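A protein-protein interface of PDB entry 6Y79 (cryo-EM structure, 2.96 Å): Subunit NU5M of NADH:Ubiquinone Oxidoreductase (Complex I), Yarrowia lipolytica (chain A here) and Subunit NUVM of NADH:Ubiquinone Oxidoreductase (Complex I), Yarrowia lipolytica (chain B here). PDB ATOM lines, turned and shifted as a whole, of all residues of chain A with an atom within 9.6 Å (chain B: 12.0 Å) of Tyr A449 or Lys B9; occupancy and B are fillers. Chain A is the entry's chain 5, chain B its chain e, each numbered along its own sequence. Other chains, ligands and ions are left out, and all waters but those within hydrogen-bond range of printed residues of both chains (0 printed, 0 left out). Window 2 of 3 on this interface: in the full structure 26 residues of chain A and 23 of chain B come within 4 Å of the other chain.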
ATOM      1  N   SER A 352      -7.959  19.169 -26.100  1.00  0.00           N
ATOM      2  CA  SER A 352      -8.644  17.931 -26.440  1.00  0.00           C
ATOM      3  C   SER A 352      -8.025  16.724 -25.747  1.00  0.00           C
ATOM      4  O   SER A 352      -8.734  15.768 -25.425  1.00  0.00           O
ATOM      5  CB  SER A 352      -8.637  17.741 -27.954  1.00  0.00           C
ATOM      6  OG  SER A 352      -9.148  16.477 -28.316  1.00  0.00           O
ATOM      7  N   ILE A 353      -6.718  16.750 -25.507  1.00  0.00           N
ATOM      8  CA  ILE A 353      -6.052  15.668 -24.793  1.00  0.00           C
ATOM      9  C   ILE A 353      -6.437  15.721 -23.320  1.00  0.00           C
ATOM     10  O   ILE A 353      -6.404  16.789 -22.695  1.00  0.00           O
ATOM     11  CB  ILE A 353      -4.532  15.770 -25.007  1.00  0.00           C
ATOM     12  CG1 ILE A 353      -4.204  15.465 -26.464  1.00  0.00           C
ATOM     13  CG2 ILE A 353      -3.770  14.841 -24.109  1.00  0.00           C
ATOM     14  CD1 ILE A 353      -2.746  15.618 -26.796  1.00  0.00           C
ATOM     15  N   LEU A 354      -6.836  14.565 -22.769  1.00  0.00           N
ATOM     16  CA  LEU A 354      -7.168  14.446 -21.347  1.00  0.00           C
ATOM     17  C   LEU A 354      -5.980  14.787 -20.461  1.00  0.00           C
ATOM     18  O   LEU A 354      -6.156  15.329 -19.366  1.00  0.00           O
ATOM     19  CB  LEU A 354      -7.648  13.022 -21.043  1.00  0.00           C
ATOM     20  CG  LEU A 354      -8.281  12.621 -19.700  1.00  0.00           C
ATOM     21  CD1 LEU A 354      -9.280  11.513 -19.947  1.00  0.00           C
ATOM     22  CD2 LEU A 354      -7.285  12.161 -18.633  1.00  0.00           C
ATOM     23  N   GLY A 365      -0.399  10.191 -33.210  1.00  0.00           N
ATOM     24  CA  GLY A 365      -1.294  10.479 -34.314  1.00  0.00           C
ATOM     25  C   GLY A 365      -2.686  10.840 -33.831  1.00  0.00           C
ATOM     26  O   GLY A 365      -3.231  10.220 -32.921  1.00  0.00           O
ATOM     27  N   LEU A 366      -3.251  11.888 -34.435  1.00  0.00           N
ATOM     28  CA  LEU A 366      -4.590  12.352 -34.097  1.00  0.00           C
ATOM     29  C   LEU A 366      -5.363  12.783 -35.333  1.00  0.00           C
ATOM     30  O   LEU A 366      -6.294  13.587 -35.232  1.00  0.00           O
ATOM     31  CB  LEU A 366      -4.544  13.522 -33.115  1.00  0.00           C
ATOM     32  CG  LEU A 366      -4.061  13.311 -31.686  1.00  0.00           C
ATOM     33  CD1 LEU A 366      -3.903  14.652 -31.007  1.00  0.00           C
ATOM     34  CD2 LEU A 366      -5.039  12.447 -30.934  1.00  0.00           C
ATOM     35  N   TYR A 369      -8.891  11.363 -35.321  1.00  0.00           N
ATOM     36  CA  TYR A 369      -9.706  11.781 -34.189  1.00  0.00           C
ATOM     37  C   TYR A 369     -10.055  13.257 -34.231  1.00  0.00           C
ATOM     38  O   TYR A 369     -11.100  13.657 -33.708  1.00  0.00           O
ATOM     39  CB  TYR A 369      -8.974  11.466 -32.882  1.00  0.00           C
ATOM     40  CG  TYR A 369      -8.768   9.989 -32.609  1.00  0.00           C
ATOM     41  CD1 TYR A 369      -9.517   9.029 -33.254  1.00  0.00           C
ATOM     42  CD2 TYR A 369      -7.808   9.556 -31.723  1.00  0.00           C
ATOM     43  CE1 TYR A 369      -9.340   7.685 -33.015  1.00  0.00           C
ATOM     44  CE2 TYR A 369      -7.626   8.209 -31.486  1.00  0.00           C
ATOM     45  CZ  TYR A 369      -8.391   7.281 -32.129  1.00  0.00           C
ATOM     46  OH  TYR A 369      -8.198   5.941 -31.885  1.00  0.00           O
ATOM     47  N   LEU A 370      -9.197  14.081 -34.825  1.00  0.00           N
ATOM     48  CA  LEU A 370      -9.365  15.532 -34.830  1.00  0.00           C
ATOM     49  C   LEU A 370      -9.224  16.067 -36.250  1.00  0.00           C
ATOM     50  O   LEU A 370      -8.210  16.686 -36.586  1.00  0.00           O
ATOM     51  CB  LEU A 370      -8.345  16.185 -33.899  1.00  0.00           C
ATOM     52  CG  LEU A 370      -8.676  16.230 -32.409  1.00  0.00           C
ATOM     53  CD1 LEU A 370      -8.329  14.951 -31.693  1.00  0.00           C
ATOM     54  CD2 LEU A 370      -7.943  17.357 -31.766  1.00  0.00           C
ATOM     55  N   ASN A 443       0.893   8.482 -26.830  1.00  0.00           N
ATOM     56  CA  ASN A 443       0.206   8.603 -25.559  1.00  0.00           C
ATOM     57  C   ASN A 443      -0.433   7.273 -25.175  1.00  0.00           C
ATOM     58  O   ASN A 443      -0.479   6.327 -25.963  1.00  0.00           O
ATOM     59  CB  ASN A 443      -0.846   9.705 -25.633  1.00  0.00           C
ATOM     60  CG  ASN A 443      -0.991  10.458 -24.332  1.00  0.00           C
ATOM     61  OD1 ASN A 443      -0.494  10.031 -23.294  1.00  0.00           O
ATOM     62  ND2 ASN A 443      -1.654  11.599 -24.387  1.00  0.00           N
ATOM     63  N   ASN A 444      -0.926   7.199 -23.941  1.00  0.00           N
ATOM     64  CA  ASN A 444      -1.629   5.999 -23.514  1.00  0.00           C
ATOM     65  C   ASN A 444      -3.013   5.942 -24.159  1.00  0.00           C
ATOM     66  O   ASN A 444      -3.510   6.926 -24.712  1.00  0.00           O
ATOM     67  CB  ASN A 444      -1.717   5.933 -21.988  1.00  0.00           C
ATOM     68  CG  ASN A 444      -2.374   7.154 -21.369  1.00  0.00           C
ATOM     69  OD1 ASN A 444      -2.747   8.105 -22.050  1.00  0.00           O
ATOM     70  ND2 ASN A 444      -2.523   7.123 -20.053  1.00  0.00           N
ATOM     71  N   THR A 445      -3.646   4.771 -24.063  1.00  0.00           N
ATOM     72  CA  THR A 445      -4.813   4.472 -24.888  1.00  0.00           C
ATOM     73  C   THR A 445      -6.051   5.267 -24.490  1.00  0.00           C
ATOM     74  O   THR A 445      -6.916   5.517 -25.338  1.00  0.00           O
ATOM     75  CB  THR A 445      -5.101   2.965 -24.843  1.00  0.00           C
ATOM     76  OG1 THR A 445      -6.187   2.655 -25.718  1.00  0.00           O
ATOM     77  CG2 THR A 445      -5.431   2.490 -23.430  1.00  0.00           C
ATOM     78  N   ILE A 446      -6.116   5.734 -23.246  1.00  0.00           N
ATOM     79  CA  ILE A 446      -7.337   6.337 -22.739  1.00  0.00           C
ATOM     80  C   ILE A 446      -7.516   7.764 -23.258  1.00  0.00           C
ATOM     81  O   ILE A 446      -8.652   8.226 -23.439  1.00  0.00           O
ATOM     82  CB  ILE A 446      -7.321   6.261 -21.207  1.00  0.00           C
ATOM     83  CG1 ILE A 446      -8.636   6.764 -20.639  1.00  0.00           C
ATOM     84  CG2 ILE A 446      -6.108   6.978 -20.616  1.00  0.00           C
ATOM     85  CD1 ILE A 446      -8.673   6.680 -19.213  1.00  0.00           C
ATOM     86  N   THR A 447      -6.412   8.466 -23.529  1.00  0.00           N
ATOM     87  CA  THR A 447      -6.445   9.719 -24.266  1.00  0.00           C
ATOM     88  C   THR A 447      -7.079   9.543 -25.633  1.00  0.00           C
ATOM     89  O   THR A 447      -7.908  10.362 -26.042  1.00  0.00           O
ATOM     90  CB  THR A 447      -5.021  10.248 -24.415  1.00  0.00           C
ATOM     91  OG1 THR A 447      -4.462  10.485 -23.117  1.00  0.00           O
ATOM     92  CG2 THR A 447      -5.001  11.528 -25.204  1.00  0.00           C
ATOM     93  N   TYR A 448      -6.760   8.448 -26.307  1.00  0.00           N
ATOM     94  CA  TYR A 448      -7.347   8.170 -27.603  1.00  0.00           C
ATOM     95  C   TYR A 448      -8.792   7.704 -27.488  1.00  0.00           C
ATOM     96  O   TYR A 448      -9.553   7.827 -28.454  1.00  0.00           O
ATOM     97  CB  TYR A 448      -6.467   7.155 -28.325  1.00  0.00           C
ATOM     98  CG  TYR A 448      -5.090   7.713 -28.597  1.00  0.00           C
ATOM     99  CD1 TYR A 448      -4.899   8.681 -29.569  1.00  0.00           C
ATOM    100  CD2 TYR A 448      -3.989   7.298 -27.868  1.00  0.00           C
ATOM    101  CE1 TYR A 448      -3.663   9.205 -29.828  1.00  0.00           C
ATOM    102  CE2 TYR A 448      -2.737   7.824 -28.119  1.00  0.00           C
ATOM    103  CZ  TYR A 448      -2.588   8.781 -29.100  1.00  0.00           C
ATOM    104  OH  TYR A 448      -1.356   9.317 -29.370  1.00  0.00           O
ATOM    105  N   TYR A 449      -9.199   7.176 -26.329  1.00  0.00           N
ATOM    106  CA  TYR A 449     -10.628   6.949 -26.110  1.00  0.00           C
ATOM    107  C   TYR A 449     -11.380   8.260 -25.932  1.00  0.00           C
ATOM    108  O   TYR A 449     -12.481   8.427 -26.468  1.00  0.00           O
ATOM    109  CB  TYR A 449     -10.867   6.058 -24.892  1.00  0.00           C
ATOM    110  CG  TYR A 449     -10.564   4.604 -25.124  1.00  0.00           C
ATOM    111  CD1 TYR A 449     -11.339   3.836 -25.983  1.00  0.00           C
ATOM    112  CD2 TYR A 449      -9.511   3.995 -24.468  1.00  0.00           C
ATOM    113  CE1 TYR A 449     -11.056   2.505 -26.187  1.00  0.00           C
ATOM    114  CE2 TYR A 449      -9.217   2.677 -24.668  1.00  0.00           C
ATOM    115  CZ  TYR A 449      -9.989   1.938 -25.529  1.00  0.00           C
ATOM    116  OH  TYR A 449      -9.687   0.618 -25.721  1.00  0.00           O
ATOM    117  N   ASN A 450     -10.808   9.197 -25.181  1.00  0.00           N
ATOM    118  CA  ASN A 450     -11.512  10.403 -24.771  1.00  0.00           C
ATOM    119  C   ASN A 450     -11.218  11.605 -25.658  1.00  0.00           C
ATOM    120  O   ASN A 450     -11.645  12.716 -25.327  1.00  0.00           O
ATOM    121  CB  ASN A 450     -11.169  10.742 -23.322  1.00  0.00           C
ATOM    122  CG  ASN A 450     -11.648   9.688 -22.354  1.00  0.00           C
ATOM    123  OD1 ASN A 450     -10.853   9.073 -21.647  1.00  0.00           O
ATOM    124  ND2 ASN A 450     -12.954   9.470 -22.317  1.00  0.00           N
ATOM    125  N   ALA A 451     -10.505  11.420 -26.764  1.00  0.00           N
ATOM    126  CA  ALA A 451     -10.264  12.523 -27.684  1.00  0.00           C
ATOM    127  C   ALA A 451     -11.536  12.826 -28.459  1.00  0.00           C
ATOM    128  O   ALA A 451     -12.041  11.981 -29.205  1.00  0.00           O
ATOM    129  CB  ALA A 451      -9.120  12.195 -28.636  1.00  0.00           C
ATOM    130  N   HIS A 452     -12.054  14.031 -28.267  1.00  0.00           N
ATOM    131  CA  HIS A 452     -13.240  14.512 -28.951  1.00  0.00           C
ATOM    132  C   HIS A 452     -12.958  15.935 -29.391  1.00  0.00           C
ATOM    133  O   HIS A 452     -11.914  16.507 -29.068  1.00  0.00           O
ATOM    134  CB  HIS A 452     -14.477  14.445 -28.046  1.00  0.00           C
ATOM    135  CG  HIS A 452     -14.360  15.286 -26.816  1.00  0.00           C
ATOM    136  ND1 HIS A 452     -13.558  14.938 -25.750  1.00  0.00           N
ATOM    137  CD2 HIS A 452     -14.928  16.468 -26.486  1.00  0.00           C
ATOM    138  CE1 HIS A 452     -13.640  15.868 -24.817  1.00  0.00           C
ATOM    139  NE2 HIS A 452     -14.464  16.807 -25.238  1.00  0.00           N
ATOM    140  N   GLU A 453     -13.883  16.499 -30.156  1.00  0.00           N
ATOM    141  CA  GLU A 453     -13.703  17.868 -30.603  1.00  0.00           C
ATOM    142  C   GLU A 453     -14.468  18.855 -29.731  1.00  0.00           C
ATOM    143  O   GLU A 453     -15.496  18.541 -29.133  1.00  0.00           O
ATOM    144  CB  GLU A 453     -14.076  18.015 -32.076  1.00  0.00           C
ATOM    145  CG  GLU A 453     -12.936  17.523 -32.927  1.00  0.00           C
ATOM    146  CD  GLU A 453     -13.069  17.956 -34.357  1.00  0.00           C
ATOM    147  OE1 GLU A 453     -14.079  18.609 -34.675  1.00  0.00           O
ATOM    148  OE2 GLU A 453     -12.164  17.649 -35.147  1.00  0.00           O
ATOM    149  N   ASN B   7     -14.161   3.105 -22.825  1.00  0.00           N
ATOM    150  CA  ASN B   7     -12.966   2.640 -22.135  1.00  0.00           C
ATOM    151  C   ASN B   7     -12.750   1.148 -22.315  1.00  0.00           C
ATOM    152  O   ASN B   7     -11.760   0.619 -21.830  1.00  0.00           O
ATOM    153  CB  ASN B   7     -13.046   2.935 -20.632  1.00  0.00           C
ATOM    154  CG  ASN B   7     -13.592   4.313 -20.328  1.00  0.00           C
ATOM    155  OD1 ASN B   7     -12.838   5.281 -20.231  1.00  0.00           O
ATOM    156  ND2 ASN B   7     -14.905   4.406 -20.146  1.00  0.00           N
ATOM    157  N   TYR B   8     -13.649   0.499 -23.062  1.00  0.00           N
ATOM    158  CA  TYR B   8     -13.978  -0.909 -22.836  1.00  0.00           C
ATOM    159  C   TYR B   8     -12.827  -1.872 -23.109  1.00  0.00           C
ATOM    160  O   TYR B   8     -12.817  -2.975 -22.553  1.00  0.00           O
ATOM    161  CB  TYR B   8     -15.187  -1.306 -23.683  1.00  0.00           C
ATOM    162  CG  TYR B   8     -16.482  -0.624 -23.284  1.00  0.00           C
ATOM    163  CD1 TYR B   8     -16.630  -0.028 -22.032  1.00  0.00           C
ATOM    164  CD2 TYR B   8     -17.557  -0.574 -24.161  1.00  0.00           C
ATOM    165  CE1 TYR B   8     -17.801   0.599 -21.671  1.00  0.00           C
ATOM    166  CE2 TYR B   8     -18.737   0.048 -23.807  1.00  0.00           C
ATOM    167  CZ  TYR B   8     -18.853   0.634 -22.560  1.00  0.00           C
ATOM    168  OH  TYR B   8     -20.027   1.259 -22.200  1.00  0.00           O
ATOM    169  N   LYS B   9     -11.856  -1.489 -23.928  1.00  0.00           N
ATOM    170  CA  LYS B   9     -10.672  -2.303 -24.140  1.00  0.00           C
ATOM    171  C   LYS B   9      -9.452  -1.607 -23.557  1.00  0.00           C
ATOM    172  O   LYS B   9      -9.424  -0.382 -23.414  1.00  0.00           O
ATOM    173  CB  LYS B   9     -10.433  -2.572 -25.624  1.00  0.00           C
ATOM    174  CG  LYS B   9     -11.576  -3.246 -26.338  1.00  0.00           C
ATOM    175  CD  LYS B   9     -11.232  -3.414 -27.799  1.00  0.00           C
ATOM    176  CE  LYS B   9     -12.298  -4.181 -28.554  1.00  0.00           C
ATOM    177  NZ  LYS B   9     -11.954  -4.310 -29.999  1.00  0.00           N
ATOM    178  N   TRP B  10      -8.443  -2.398 -23.215  1.00  0.00           N
ATOM    179  CA  TRP B  10      -7.149  -1.859 -22.844  1.00  0.00           C
ATOM    180  C   TRP B  10      -6.047  -2.618 -23.559  1.00  0.00           C
ATOM    181  O   TRP B  10      -6.093  -3.848 -23.681  1.00  0.00           O
ATOM    182  CB  TRP B  10      -6.933  -1.905 -21.330  1.00  0.00           C
ATOM    183  CG  TRP B  10      -7.748  -0.877 -20.643  1.00  0.00           C
ATOM    184  CD1 TRP B  10      -7.415   0.429 -20.433  1.00  0.00           C
ATOM    185  CD2 TRP B  10      -9.052  -1.051 -20.095  1.00  0.00           C
ATOM    186  NE1 TRP B  10      -8.437   1.080 -19.793  1.00  0.00           N
ATOM    187  CE2 TRP B  10      -9.449   0.188 -19.560  1.00  0.00           C
ATOM    188  CE3 TRP B  10      -9.922  -2.137 -19.999  1.00  0.00           C
ATOM    189  CZ2 TRP B  10     -10.674   0.369 -18.929  1.00  0.00           C
ATOM    190  CZ3 TRP B  10     -11.140  -1.954 -19.384  1.00  0.00           C
ATOM    191  CH2 TRP B  10     -11.509  -0.709 -18.863  1.00  0.00           C
ATOM    192  N   ASN B  11      -5.061  -1.834 -24.020  1.00  0.00           N
ATOM    193  CA  ASN B  11      -3.864  -2.243 -24.752  1.00  0.00           C
ATOM    194  C   ASN B  11      -4.164  -3.270 -25.838  1.00  0.00           C
ATOM    195  O   ASN B  11      -3.464  -4.274 -25.990  1.00  0.00           O
ATOM    196  CB  ASN B  11      -2.810  -2.735 -23.760  1.00  0.00           C
ATOM    197  CG  ASN B  11      -2.298  -1.610 -22.880  1.00  0.00           C
ATOM    198  OD1 ASN B  11      -2.900  -0.535 -22.841  1.00  0.00           O
ATOM    199  ND2 ASN B  11      -1.189  -1.839 -22.181  1.00  0.00           N
ATOM    200  N   GLY B  12      -5.228  -3.002 -26.584  1.00  0.00           N
ATOM    201  CA  GLY B  12      -5.628  -3.772 -27.733  1.00  0.00           C
ATOM    202  C   GLY B  12      -6.284  -2.809 -28.694  1.00  0.00           C
ATOM    203  O   GLY B  12      -6.287  -1.599 -28.449  1.00  0.00           O
ATOM    204  N   PRO B  13      -6.880  -3.320 -29.774  1.00  0.00           N
ATOM    205  CA  PRO B  13      -7.271  -2.462 -30.906  1.00  0.00           C
ATOM    206  C   PRO B  13      -8.370  -1.467 -30.557  1.00  0.00           C
ATOM    207  O   PRO B  13      -9.408  -1.827 -30.001  1.00  0.00           O
ATOM    208  CB  PRO B  13      -7.748  -3.465 -31.962  1.00  0.00           C
ATOM    209  CG  PRO B  13      -7.267  -4.797 -31.502  1.00  0.00           C
ATOM    210  CD  PRO B  13      -7.207  -4.733 -30.019  1.00  0.00           C
ATOM    211  N   LEU B  14      -8.125  -0.203 -30.891  1.00  0.00           N
ATOM    212  CA  LEU B  14      -9.047   0.873 -30.583  1.00  0.00           C
ATOM    213  C   LEU B  14     -10.258   0.793 -31.512  1.00  0.00           C
ATOM    214  O   LEU B  14     -10.229   0.088 -32.519  1.00  0.00           O
ATOM    215  CB  LEU B  14      -8.336   2.218 -30.729  1.00  0.00           C
ATOM    216  CG  LEU B  14      -7.549   2.871 -29.577  1.00  0.00           C
ATOM    217  CD1 LEU B  14      -8.474   3.395 -28.504  1.00  0.00           C
ATOM    218  CD2 LEU B  14      -6.502   1.951 -28.964  1.00  0.00           C
ATOM    219  N   PRO B  15     -11.359   1.451 -31.177  1.00  0.00           N
ATOM    220  CA  PRO B  15     -12.439   1.588 -32.157  1.00  0.00           C
ATOM    221  C   PRO B  15     -12.188   2.748 -33.108  1.00  0.00           C
ATOM    222  O   PRO B  15     -11.378   3.640 -32.854  1.00  0.00           O
ATOM    223  CB  PRO B  15     -13.678   1.838 -31.293  1.00  0.00           C
ATOM    224  CG  PRO B  15     -13.143   2.419 -30.044  1.00  0.00           C
ATOM    225  CD  PRO B  15     -11.824   1.757 -29.813  1.00  0.00           C
ATOM    226  N   ARG B  16     -12.881   2.699 -34.242  1.00  0.00           N
ATOM    227  CA  ARG B  16     -12.943   3.859 -35.121  1.00  0.00           C
ATOM    228  C   ARG B  16     -13.736   4.963 -34.425  1.00  0.00           C
ATOM    229  O   ARG B  16     -14.754   4.681 -33.788  1.00  0.00           O
ATOM    230  CB  ARG B  16     -13.594   3.484 -36.461  1.00  0.00           C
ATOM    231  CG  ARG B  16     -13.704   4.634 -37.451  1.00  0.00           C
ATOM    232  CD  ARG B  16     -14.093   4.230 -38.852  1.00  0.00           C
ATOM    233  NE  ARG B  16     -14.157   5.406 -39.716  1.00  0.00           N
ATOM    234  CZ  ARG B  16     -13.116   5.912 -40.375  1.00  0.00           C
ATOM    235  NH1 ARG B  16     -11.923   5.337 -40.284  1.00  0.00           N
ATOM    236  NH2 ARG B  16     -13.267   6.988 -41.134  1.00  0.00           N
ATOM    237  N   PRO B  17     -13.279   6.214 -34.488  1.00  0.00           N
ATOM    238  CA  PRO B  17     -13.903   7.265 -33.686  1.00  0.00           C
ATOM    239  C   PRO B  17     -15.275   7.685 -34.173  1.00  0.00           C
ATOM    240  O   PRO B  17     -15.710   7.426 -35.301  1.00  0.00           O
ATOM    241  CB  PRO B  17     -12.928   8.431 -33.821  1.00  0.00           C
ATOM    242  CG  PRO B  17     -12.327   8.200 -35.149  1.00  0.00           C
ATOM    243  CD  PRO B  17     -12.057   6.734 -35.114  1.00  0.00           C
ATOM    244  N   HIS B  18     -15.933   8.391 -33.272  1.00  0.00           N
ATOM    245  CA  HIS B  18     -17.249   8.978 -33.467  1.00  0.00           C
ATOM    246  C   HIS B  18     -17.038  10.474 -33.570  1.00  0.00           C
ATOM    247  O   HIS B  18     -16.758  11.130 -32.575  1.00  0.00           O
ATOM    248  CB  HIS B  18     -18.143   8.607 -32.297  1.00  0.00           C
ATOM    249  CG  HIS B  18     -19.555   9.087 -32.386  1.00  0.00           C
ATOM    250  ND1 HIS B  18     -19.926  10.363 -32.027  1.00  0.00           N
ATOM    251  CD2 HIS B  18     -20.697   8.433 -32.707  1.00  0.00           C
ATOM    252  CE1 HIS B  18     -21.233  10.490 -32.167  1.00  0.00           C
ATOM    253  NE2 HIS B  18     -21.724   9.333 -32.576  1.00  0.00           N
ATOM    254  N   VAL B  19     -17.093  10.998 -34.763  1.00  0.00           N
ATOM    255  CA  VAL B  19     -17.153  12.443 -34.962  1.00  0.00           C
ATOM    256  C   VAL B  19     -18.569  12.776 -35.418  1.00  0.00           C
ATOM    257  O   VAL B  19     -19.313  11.891 -35.885  1.00  0.00           O
ATOM    258  CB  VAL B  19     -16.078  12.929 -35.962  1.00  0.00           C
ATOM    259  CG1 VAL B  19     -16.527  12.742 -37.401  1.00  0.00           C
ATOM    260  CG2 VAL B  19     -15.673  14.357 -35.668  1.00  0.00           C
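Of the 13 printed residues of chain B, 5 touch a printed residue of chain A.
Hydrophobic or aromatic side chains of chain B that line the printed part of chain A: Leu B14, Pro B15 and Pro B17.
The backbone carbonyl oxygen of Lys B9 lies within hydrogen-bond range of the side-chain hydroxyl of Tyr A449, at 2.5 Å.
Of the printed residues of chain B, Thr A445 touches Asn B11 and Leu B14.
No residue of chain B comes within 4 Å of Ile A446.
No residue of chain B comes within 4 Å of Thr A447.
Of the printed residues of chain B, Tyr A449 touches Lys B9 (2.5 Å), Leu B14 (3.6 Å) and Pro B15 (3.8 Å).
No residue of chain B comes within 4 Å of Asn A450.
No residue of chain B comes within 4 Å of Ala A451.
Lys B9 touches just one residue of chain A: Tyr A449.
Gly B12 touches none of the printed residues of chain A.
Of the printed residues of chain A, Leu B14 touches Tyr A369 (3.9 Å), Thr A445 (3.3 Å) and Tyr A449 (3.6 Å).
Printed residues of chain A within 4 Å of Pro B15: Tyr A449.
Of the printed residues of chain A, Pro B17 touches Tyr A369.
Val B19 touches none of the printed residues of chain A.
The nearest printed residue of chain A that does not touch Pro B15 is Tyr A369 (4.04 Å).
Leu B14 touches Tyr A369.
CG of Pro B17 touches CD1 of Tyr A369 (3.5 Å).
OD1 of Asn B11 touches CG2 of Thr A445 (3.99 Å).
CD2 of Leu B14 touches OG1 of Thr A445, at 3.3 Å.
Tyr A449 touches Leu B14.
CD of Pro B15 touches CE1 of Tyr A449, 3.8 Å away.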
